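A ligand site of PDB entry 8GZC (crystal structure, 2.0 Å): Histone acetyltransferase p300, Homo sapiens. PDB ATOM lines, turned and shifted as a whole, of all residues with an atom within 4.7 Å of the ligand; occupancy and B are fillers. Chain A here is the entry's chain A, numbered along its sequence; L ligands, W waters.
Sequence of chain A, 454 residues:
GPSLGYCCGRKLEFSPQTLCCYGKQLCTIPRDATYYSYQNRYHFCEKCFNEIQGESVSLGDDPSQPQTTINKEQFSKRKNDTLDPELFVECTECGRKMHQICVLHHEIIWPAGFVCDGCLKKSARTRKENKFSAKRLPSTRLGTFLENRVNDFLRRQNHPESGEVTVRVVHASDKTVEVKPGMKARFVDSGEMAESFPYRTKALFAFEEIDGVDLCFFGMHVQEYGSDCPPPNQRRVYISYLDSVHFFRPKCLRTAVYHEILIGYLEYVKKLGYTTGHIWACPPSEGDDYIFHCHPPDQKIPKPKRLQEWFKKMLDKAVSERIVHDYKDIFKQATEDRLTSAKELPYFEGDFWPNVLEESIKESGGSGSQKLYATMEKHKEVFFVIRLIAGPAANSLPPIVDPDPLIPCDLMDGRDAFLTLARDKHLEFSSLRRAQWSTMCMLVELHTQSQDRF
Water W1 lies within hydrogen-bond range of N of Tyr 290, N3 of the ligand and OD2 of Asp 243.
Water W4 lies within hydrogen-bond range of O1 of the ligand (2.9 Å), NE2 of Gln 299 (3.2 Å) and O of Lys 300 (3.4 Å).
Water W3 bridges a nitrogen (N4) of the ligand and the backbone carbonyl oxygen (O) of Gln 299.
Water W2 lies within hydrogen-bond range of OD1 of Asp 289, N of His 295 and N5 of the ligand.
Residues that only touch the ligand: Pro 302 (3.3 Å), His 295 (3.3 Å), Pro 284 (3.4 Å), Gln 299 (3.4 Å), Ile 301 (3.4 Å), Asp 288 (3.5 Å), Trp 310 (3.5 Å), Asp 289 (3.5 Å), Leu 242 (3.6 Å), Leu 307 (3.7 Å), Tyr 258 (3.7 Å), Arg 306 (3.9 Å) and Phe 218 (3.9 Å).
15 residues have an atom within 4 Å of the ligand: Phe 218, Leu 242, Asp 243, Ser 244, Tyr 258, Pro 284, Asp 288, Asp 289, His 295, Gln 299, Ile 301, Pro 302, Arg 306, Leu 307 and Trp 310.
O of Ser 244 is in hydrogen-bond range of NE2 of His 295, at 3.2 Å.
NE2 of Gln 299 lies within hydrogen-bond range of O of Ser 244, at 3.0 Å.
NE2 of His 295 lies within hydrogen-bond range of OD1 of Asp 243.
OD1 of Asp 289 is in hydrogen-bond range of ND1 of His 295, 2.7 Å away.
OG of Ser 244 is in hydrogen-bond range of O3 of the ligand, at 2.7 Å.
The side-chain carboxylate (OD1) of Asp 243 is in hydrogen-bond range of a nitrogen (N2) of the ligand, 3.1 Å away.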
ATOM      1  N   PHE A 218      11.333   8.244  -7.757  1.00  0.00           N
ATOM      2  CA  PHE A 218      10.039   8.799  -7.381  1.00  0.00           C
ATOM      3  C   PHE A 218       9.579   9.794  -8.446  1.00  0.00           C
ATOM      4  O   PHE A 218      10.386  10.580  -8.956  1.00  0.00           O
ATOM      5  CB  PHE A 218      10.119   9.491  -6.013  1.00  0.00           C
ATOM      6  CG  PHE A 218       8.882  10.255  -5.653  1.00  0.00           C
ATOM      7  CD1 PHE A 218       8.718  11.571  -6.032  1.00  0.00           C
ATOM      8  CD2 PHE A 218       7.869   9.643  -4.923  1.00  0.00           C
ATOM      9  CE1 PHE A 218       7.581  12.267  -5.712  1.00  0.00           C
ATOM     10  CE2 PHE A 218       6.724  10.335  -4.600  1.00  0.00           C
ATOM     11  CZ  PHE A 218       6.577  11.654  -4.993  1.00  0.00           C
ATOM     12  N   LEU A 242       1.213   9.136  -8.784  1.00  0.00           N
ATOM     13  CA  LEU A 242       2.417   8.930  -7.977  1.00  0.00           C
ATOM     14  C   LEU A 242       3.003   7.570  -8.339  1.00  0.00           C
ATOM     15  O   LEU A 242       2.259   6.611  -8.571  1.00  0.00           O
ATOM     16  CB  LEU A 242       2.117   8.952  -6.483  1.00  0.00           C
ATOM     17  CG  LEU A 242       1.701  10.282  -5.859  1.00  0.00           C
ATOM     18  CD1 LEU A 242       0.934  10.029  -4.570  1.00  0.00           C
ATOM     19  CD2 LEU A 242       2.928  11.102  -5.585  1.00  0.00           C
ATOM     20  N   ASP A 243       4.330   7.494  -8.379  1.00  0.00           N
ATOM     21  CA  ASP A 243       4.989   6.229  -8.679  1.00  0.00           C
ATOM     22  C   ASP A 243       6.376   6.235  -8.060  1.00  0.00           C
ATOM     23  O   ASP A 243       6.925   7.282  -7.720  1.00  0.00           O
ATOM     24  CB  ASP A 243       5.076   5.997 -10.194  1.00  0.00           C
ATOM     25  CG  ASP A 243       5.115   4.524 -10.557  1.00  0.00           C
ATOM     26  OD1 ASP A 243       5.173   3.685  -9.634  1.00  0.00           O
ATOM     27  OD2 ASP A 243       5.106   4.208 -11.760  1.00  0.00           O
ATOM     28  N   SER A 244       6.936   5.037  -7.916  1.00  0.00           N
ATOM     29  CA  SER A 244       8.233   4.877  -7.285  1.00  0.00           C
ATOM     30  C   SER A 244       8.910   3.622  -7.809  1.00  0.00           C
ATOM     31  O   SER A 244       8.255   2.701  -8.293  1.00  0.00           O
ATOM     32  CB  SER A 244       8.105   4.818  -5.752  1.00  0.00           C
ATOM     33  OG  SER A 244       7.492   3.608  -5.341  1.00  0.00           O
ATOM     34  N   TYR A 258       9.538   9.454   0.890  1.00  0.00           N
ATOM     35  CA  TYR A 258       8.284   9.702   0.186  1.00  0.00           C
ATOM     36  C   TYR A 258       7.425  10.703   0.958  1.00  0.00           C
ATOM     37  O   TYR A 258       6.877  11.638   0.376  1.00  0.00           O
ATOM     38  CB  TYR A 258       7.522   8.399  -0.033  1.00  0.00           C
ATOM     39  CG  TYR A 258       8.234   7.363  -0.868  1.00  0.00           C
ATOM     40  CD1 TYR A 258       9.119   7.735  -1.877  1.00  0.00           C
ATOM     41  CD2 TYR A 258       8.015   6.004  -0.654  1.00  0.00           C
ATOM     42  CE1 TYR A 258       9.771   6.770  -2.639  1.00  0.00           C
ATOM     43  CE2 TYR A 258       8.666   5.045  -1.407  1.00  0.00           C
ATOM     44  CZ  TYR A 258       9.538   5.430  -2.401  1.00  0.00           C
ATOM     45  OH  TYR A 258      10.185   4.478  -3.158  1.00  0.00           O
ATOM     46  N   LEU A 262       6.052  14.409  -0.298  1.00  0.00           N
ATOM     47  CA  LEU A 262       4.622  14.681  -0.396  1.00  0.00           C
ATOM     48  C   LEU A 262       4.170  15.717   0.616  1.00  0.00           C
ATOM     49  O   LEU A 262       3.385  16.615   0.283  1.00  0.00           O
ATOM     50  CB  LEU A 262       3.833  13.381  -0.224  1.00  0.00           C
ATOM     51  CG  LEU A 262       3.881  12.429  -1.430  1.00  0.00           C
ATOM     52  CD1 LEU A 262       3.042  11.185  -1.176  1.00  0.00           C
ATOM     53  CD2 LEU A 262       3.424  13.141  -2.690  1.00  0.00           C
ATOM     54  N   CYS A 282      -5.594   5.139  -5.327  1.00  0.00           N
ATOM     55  CA  CYS A 282      -5.963   4.075  -6.243  1.00  0.00           C
ATOM     56  C   CYS A 282      -4.731   3.327  -6.728  1.00  0.00           C
ATOM     57  O   CYS A 282      -3.883   3.917  -7.436  1.00  0.00           O
ATOM     58  CB  CYS A 282      -6.752   4.633  -7.442  1.00  0.00           C
ATOM     59  SG  CYS A 282      -7.189   3.375  -8.663  1.00  0.00           S
ATOM     60  N   PRO A 283      -4.581   2.044  -6.391  1.00  0.00           N
ATOM     61  CA  PRO A 283      -3.456   1.279  -6.926  1.00  0.00           C
ATOM     62  C   PRO A 283      -3.619   1.045  -8.409  1.00  0.00           C
ATOM     63  O   PRO A 283      -4.748   0.934  -8.916  1.00  0.00           O
ATOM     64  CB  PRO A 283      -3.524  -0.046  -6.140  1.00  0.00           C
ATOM     65  CG  PRO A 283      -4.597   0.127  -5.102  1.00  0.00           C
ATOM     66  CD  PRO A 283      -5.485   1.221  -5.573  1.00  0.00           C
ATOM     67  N   PRO A 284      -2.521   0.952  -9.158  1.00  0.00           N
ATOM     68  CA  PRO A 284      -2.616   0.479 -10.538  1.00  0.00           C
ATOM     69  C   PRO A 284      -3.020  -0.980 -10.569  1.00  0.00           C
ATOM     70  O   PRO A 284      -2.736  -1.748  -9.649  1.00  0.00           O
ATOM     71  CB  PRO A 284      -1.198   0.667 -11.074  1.00  0.00           C
ATOM     72  CG  PRO A 284      -0.332   0.550  -9.874  1.00  0.00           C
ATOM     73  CD  PRO A 284      -1.122   1.163  -8.739  1.00  0.00           C
ATOM     74  N   ASP A 288       0.116  -2.650 -15.249  1.00  0.00           N
ATOM     75  CA  ASP A 288      -0.037  -1.255 -15.616  1.00  0.00           C
ATOM     76  C   ASP A 288       0.960  -0.422 -14.835  1.00  0.00           C
ATOM     77  O   ASP A 288       1.062  -0.555 -13.602  1.00  0.00           O
ATOM     78  CB  ASP A 288      -1.468  -0.781 -15.346  1.00  0.00           C
ATOM     79  CG  ASP A 288      -1.717   0.663 -15.777  1.00  0.00           C
ATOM     80  OD1 ASP A 288      -1.120   1.097 -16.780  1.00  0.00           O
ATOM     81  OD2 ASP A 288      -2.513   1.355 -15.104  1.00  0.00           O
ATOM     82  N   ASP A 289       1.703   0.420 -15.539  1.00  0.00           N
ATOM     83  CA  ASP A 289       2.668   1.330 -14.929  1.00  0.00           C
ATOM     84  C   ASP A 289       2.107   2.745 -14.991  1.00  0.00           C
ATOM     85  O   ASP A 289       1.710   3.212 -16.063  1.00  0.00           O
ATOM     86  CB  ASP A 289       4.016   1.270 -15.659  1.00  0.00           C
ATOM     87  CG  ASP A 289       4.700  -0.077 -15.518  1.00  0.00           C
ATOM     88  OD1 ASP A 289       4.746  -0.609 -14.392  1.00  0.00           O
ATOM     89  OD2 ASP A 289       5.210  -0.583 -16.535  1.00  0.00           O
ATOM     90  N   TYR A 290       2.080   3.429 -13.839  1.00  0.00           N
ATOM     91  CA  TYR A 290       1.636   4.822 -13.840  1.00  0.00           C
ATOM     92  C   TYR A 290       2.663   5.724 -14.517  1.00  0.00           C
ATOM     93  O   TYR A 290       2.331   6.459 -15.465  1.00  0.00           O
ATOM     94  CB  TYR A 290       1.373   5.290 -12.406  1.00  0.00           C
ATOM     95  CG  TYR A 290       0.032   4.893 -11.817  1.00  0.00           C
ATOM     96  CD1 TYR A 290      -0.949   4.294 -12.595  1.00  0.00           C
ATOM     97  CD2 TYR A 290      -0.242   5.113 -10.482  1.00  0.00           C
ATOM     98  CE1 TYR A 290      -2.170   3.932 -12.047  1.00  0.00           C
ATOM     99  CE2 TYR A 290      -1.454   4.765  -9.919  1.00  0.00           C
ATOM    100  CZ  TYR A 290      -2.418   4.170 -10.710  1.00  0.00           C
ATOM    101  OH  TYR A 290      -3.626   3.819 -10.134  1.00  0.00           O
ATOM    102  N   HIS A 295       8.284  -2.123 -13.696  1.00  0.00           N
ATOM    103  CA  HIS A 295       8.675  -2.173 -12.288  1.00  0.00           C
ATOM    104  C   HIS A 295       9.372  -3.501 -11.928  1.00  0.00           C
ATOM    105  O   HIS A 295       9.206  -4.502 -12.635  1.00  0.00           O
ATOM    106  CB  HIS A 295       7.453  -2.002 -11.389  1.00  0.00           C
ATOM    107  CG  HIS A 295       6.995  -0.580 -11.258  1.00  0.00           C
ATOM    108  ND1 HIS A 295       6.187   0.017 -12.191  1.00  0.00           N
ATOM    109  CD2 HIS A 295       7.243   0.349 -10.312  1.00  0.00           C
ATOM    110  CE1 HIS A 295       5.949   1.268 -11.819  1.00  0.00           C
ATOM    111  NE2 HIS A 295       6.573   1.492 -10.680  1.00  0.00           N
ATOM    112  N   GLN A 299       8.843  -5.690  -6.358  1.00  0.00           N
ATOM    113  CA  GLN A 299       8.158  -4.488  -5.872  1.00  0.00           C
ATOM    114  C   GLN A 299       6.661  -4.689  -6.125  1.00  0.00           C
ATOM    115  O   GLN A 299       6.213  -4.662  -7.267  1.00  0.00           O
ATOM    116  CB  GLN A 299       8.657  -3.212  -6.565  1.00  0.00           C
ATOM    117  CG  GLN A 299       7.913  -1.959  -6.087  1.00  0.00           C
ATOM    118  CD  GLN A 299       8.397  -0.663  -6.710  1.00  0.00           C
ATOM    119  OE1 GLN A 299       9.390  -0.643  -7.445  1.00  0.00           O
ATOM    120  NE2 GLN A 299       7.706   0.420  -6.421  1.00  0.00           N
ATOM    121  N   LYS A 300       5.910  -4.898  -5.047  1.00  0.00           N
ATOM    122  CA  LYS A 300       4.511  -5.278  -5.150  1.00  0.00           C
ATOM    123  C   LYS A 300       3.602  -4.055  -5.199  1.00  0.00           C
ATOM    124  O   LYS A 300       3.844  -3.058  -4.511  1.00  0.00           O
ATOM    125  CB  LYS A 300       4.109  -6.161  -3.977  1.00  0.00           C
ATOM    126  CG  LYS A 300       4.895  -7.456  -3.877  1.00  0.00           C
ATOM    127  CD  LYS A 300       4.887  -8.184  -5.201  1.00  0.00           C
ATOM    128  CE  LYS A 300       5.958  -9.258  -5.223  1.00  0.00           C
ATOM    129  NZ  LYS A 300       5.782 -10.186  -6.377  1.00  0.00           N
ATOM    130  N   ILE A 301       2.557  -4.145  -6.005  1.00  0.00           N
ATOM    131  CA  ILE A 301       1.506  -3.126  -6.008  1.00  0.00           C
ATOM    132  C   ILE A 301       0.731  -3.254  -4.700  1.00  0.00           C
ATOM    133  O   ILE A 301       0.236  -4.351  -4.376  1.00  0.00           O
ATOM    134  CB  ILE A 301       0.570  -3.279  -7.216  1.00  0.00           C
ATOM    135  CG1 ILE A 301       1.366  -3.240  -8.519  1.00  0.00           C
ATOM    136  CG2 ILE A 301      -0.505  -2.192  -7.189  1.00  0.00           C
ATOM    137  CD1 ILE A 301       0.514  -3.354  -9.770  1.00  0.00           C
ATOM    138  N   PRO A 302       0.617  -2.190  -3.906  1.00  0.00           N
ATOM    139  CA  PRO A 302      -0.159  -2.286  -2.674  1.00  0.00           C
ATOM    140  C   PRO A 302      -1.633  -2.506  -2.962  1.00  0.00           C
ATOM    141  O   PRO A 302      -2.190  -1.944  -3.906  1.00  0.00           O
ATOM    142  CB  PRO A 302       0.083  -0.929  -1.998  1.00  0.00           C
ATOM    143  CG  PRO A 302       0.376  -0.011  -3.134  1.00  0.00           C
ATOM    144  CD  PRO A 302       1.154  -0.836  -4.125  1.00  0.00           C
ATOM    145  N   ARG A 306      -4.153  -1.119   2.156  1.00  0.00           N
ATOM    146  CA  ARG A 306      -2.830  -0.740   2.627  1.00  0.00           C
ATOM    147  C   ARG A 306      -2.350   0.558   1.990  1.00  0.00           C
ATOM    148  O   ARG A 306      -1.628   1.329   2.642  1.00  0.00           O
ATOM    149  CB  ARG A 306      -1.843  -1.881   2.376  1.00  0.00           C
ATOM    150  CG  ARG A 306      -2.080  -3.057   3.304  1.00  0.00           C
ATOM    151  CD  ARG A 306      -0.944  -4.056   3.274  1.00  0.00           C
ATOM    152  NE  ARG A 306       0.095  -3.764   4.252  1.00  0.00           N
ATOM    153  CZ  ARG A 306      -0.046  -3.866   5.567  1.00  0.00           C
ATOM    154  NH1 ARG A 306      -1.190  -4.247   6.115  1.00  0.00           N
ATOM    155  NH2 ARG A 306       0.990  -3.598   6.352  1.00  0.00           N
ATOM    156  N   LEU A 307      -2.742   0.822   0.747  1.00  0.00           N
ATOM    157  CA  LEU A 307      -2.459   2.127   0.150  1.00  0.00           C
ATOM    158  C   LEU A 307      -3.155   3.239   0.918  1.00  0.00           C
ATOM    159  O   LEU A 307      -2.561   4.296   1.184  1.00  0.00           O
ATOM    160  CB  LEU A 307      -2.884   2.145  -1.322  1.00  0.00           C
ATOM    161  CG  LEU A 307      -2.565   3.436  -2.072  1.00  0.00           C
ATOM    162  CD1 LEU A 307      -1.103   3.807  -1.871  1.00  0.00           C
ATOM    163  CD2 LEU A 307      -2.898   3.339  -3.568  1.00  0.00           C
ATOM    164  N   TRP A 310      -1.422   3.856   4.121  1.00  0.00           N
ATOM    165  CA  TRP A 310      -0.175   4.564   3.824  1.00  0.00           C
ATOM    166  C   TRP A 310      -0.420   6.067   3.693  1.00  0.00           C
ATOM    167  O   TRP A 310       0.310   6.876   4.266  1.00  0.00           O
ATOM    168  CB  TRP A 310       0.449   3.995   2.558  1.00  0.00           C
ATOM    169  CG  TRP A 310       1.837   4.468   2.294  1.00  0.00           C
ATOM    170  CD1 TRP A 310       2.998   3.852   2.667  1.00  0.00           C
ATOM    171  CD2 TRP A 310       2.217   5.660   1.602  1.00  0.00           C
ATOM    172  NE1 TRP A 310       4.079   4.585   2.250  1.00  0.00           N
ATOM    173  CE2 TRP A 310       3.629   5.709   1.596  1.00  0.00           C
ATOM    174  CE3 TRP A 310       1.514   6.695   0.995  1.00  0.00           C
ATOM    175  CZ2 TRP A 310       4.345   6.742   1.000  1.00  0.00           C
ATOM    176  CZ3 TRP A 310       2.220   7.729   0.410  1.00  0.00           C
ATOM    177  CH2 TRP A 310       3.616   7.746   0.410  1.00  0.00           C
HETATM  178  N1  LIG L   1       2.558   3.788  -5.197  1.00  0.00           N
HETATM  179  C1  LIG L   1       2.686   3.316  -6.585  1.00  0.00           C
HETATM  180  C2  LIG L   1       3.084   1.984  -6.747  1.00  0.00           C
HETATM  181  O1  LIG L   1       3.126   1.227  -5.779  1.00  0.00           O
HETATM  182  C3  LIG L   1       1.304   3.477  -7.103  1.00  0.00           C
HETATM  183  C4  LIG L   1       0.378   3.156  -5.986  1.00  0.00           C
HETATM  184  C5  LIG L   1       1.100   3.757  -4.844  1.00  0.00           C
HETATM  185  C6  LIG L   1       3.962   1.257  -1.698  1.00  0.00           C
HETATM  186  C7  LIG L   1       4.224   2.357  -2.489  1.00  0.00           C
HETATM  187  C8  LIG L   1       3.513   3.532  -2.335  1.00  0.00           C
HETATM  188  C9  LIG L   1       2.518   3.593  -1.369  1.00  0.00           C
HETATM  189  C10 LIG L   1       2.252   2.476  -0.580  1.00  0.00           C
HETATM  190  C11 LIG L   1       2.981   1.314  -0.730  1.00  0.00           C
HETATM  191  C12 LIG L   1       1.834   0.535   1.087  1.00  0.00           C
HETATM  192  C13 LIG L   1       3.784   4.621  -3.154  1.00  0.00           C
HETATM  193  C14 LIG L   1       5.198   5.081  -2.843  1.00  0.00           C
HETATM  194  C15 LIG L   1       5.551   6.453  -3.444  1.00  0.00           C
HETATM  195  C16 LIG L   1       4.531   7.481  -3.128  1.00  0.00           C
HETATM  196  C17 LIG L   1       3.202   6.976  -3.584  1.00  0.00           C
HETATM  197  C18 LIG L   1       2.854   5.766  -2.801  1.00  0.00           C
HETATM  198  C19 LIG L   1       3.734   4.144  -4.634  1.00  0.00           C
HETATM  199  C20 LIG L   1       3.791   0.451  -8.427  1.00  0.00           C
HETATM  200  C21 LIG L   1       3.680  -1.096 -10.146  1.00  0.00           C
HETATM  201  C22 LIG L   1       4.397  -1.981  -9.475  1.00  0.00           C
HETATM  202  C23 LIG L   1       4.837  -1.709  -8.262  1.00  0.00           C
HETATM  203  C24 LIG L   1       4.558  -0.469  -7.711  1.00  0.00           C
HETATM  204  C25 LIG L   1       3.405  -1.689 -11.297  1.00  0.00           C
HETATM  205  F1  LIG L   1       0.416   1.892  -5.834  1.00  0.00           F
HETATM  206  N2  LIG L   1       3.441   1.670  -8.015  1.00  0.00           N
HETATM  207  N3  LIG L   1       3.380   0.089  -9.644  1.00  0.00           N
HETATM  208  N4  LIG L   1       4.497  -3.051 -10.242  1.00  0.00           N
HETATM  209  N5  LIG L   1       3.960  -2.886 -11.257  1.00  0.00           N
HETATM  210  O2  LIG L   1       2.741   0.224   0.033  1.00  0.00           O
HETATM  211  O3  LIG L   1       4.779   4.013  -5.258  1.00  0.00           O
HETATM  212  O   HOH W   1       2.728   2.075 -11.525  1.00  0.00           O
HETATM  213  O   HOH W   2       5.490  -3.222 -14.329  1.00  0.00           O
HETATM  214  O   HOH W   3       6.060  -5.648 -10.268  1.00  0.00           O
HETATM  215  O   HOH W   4       5.316  -0.040  -4.323  1.00  0.00           O
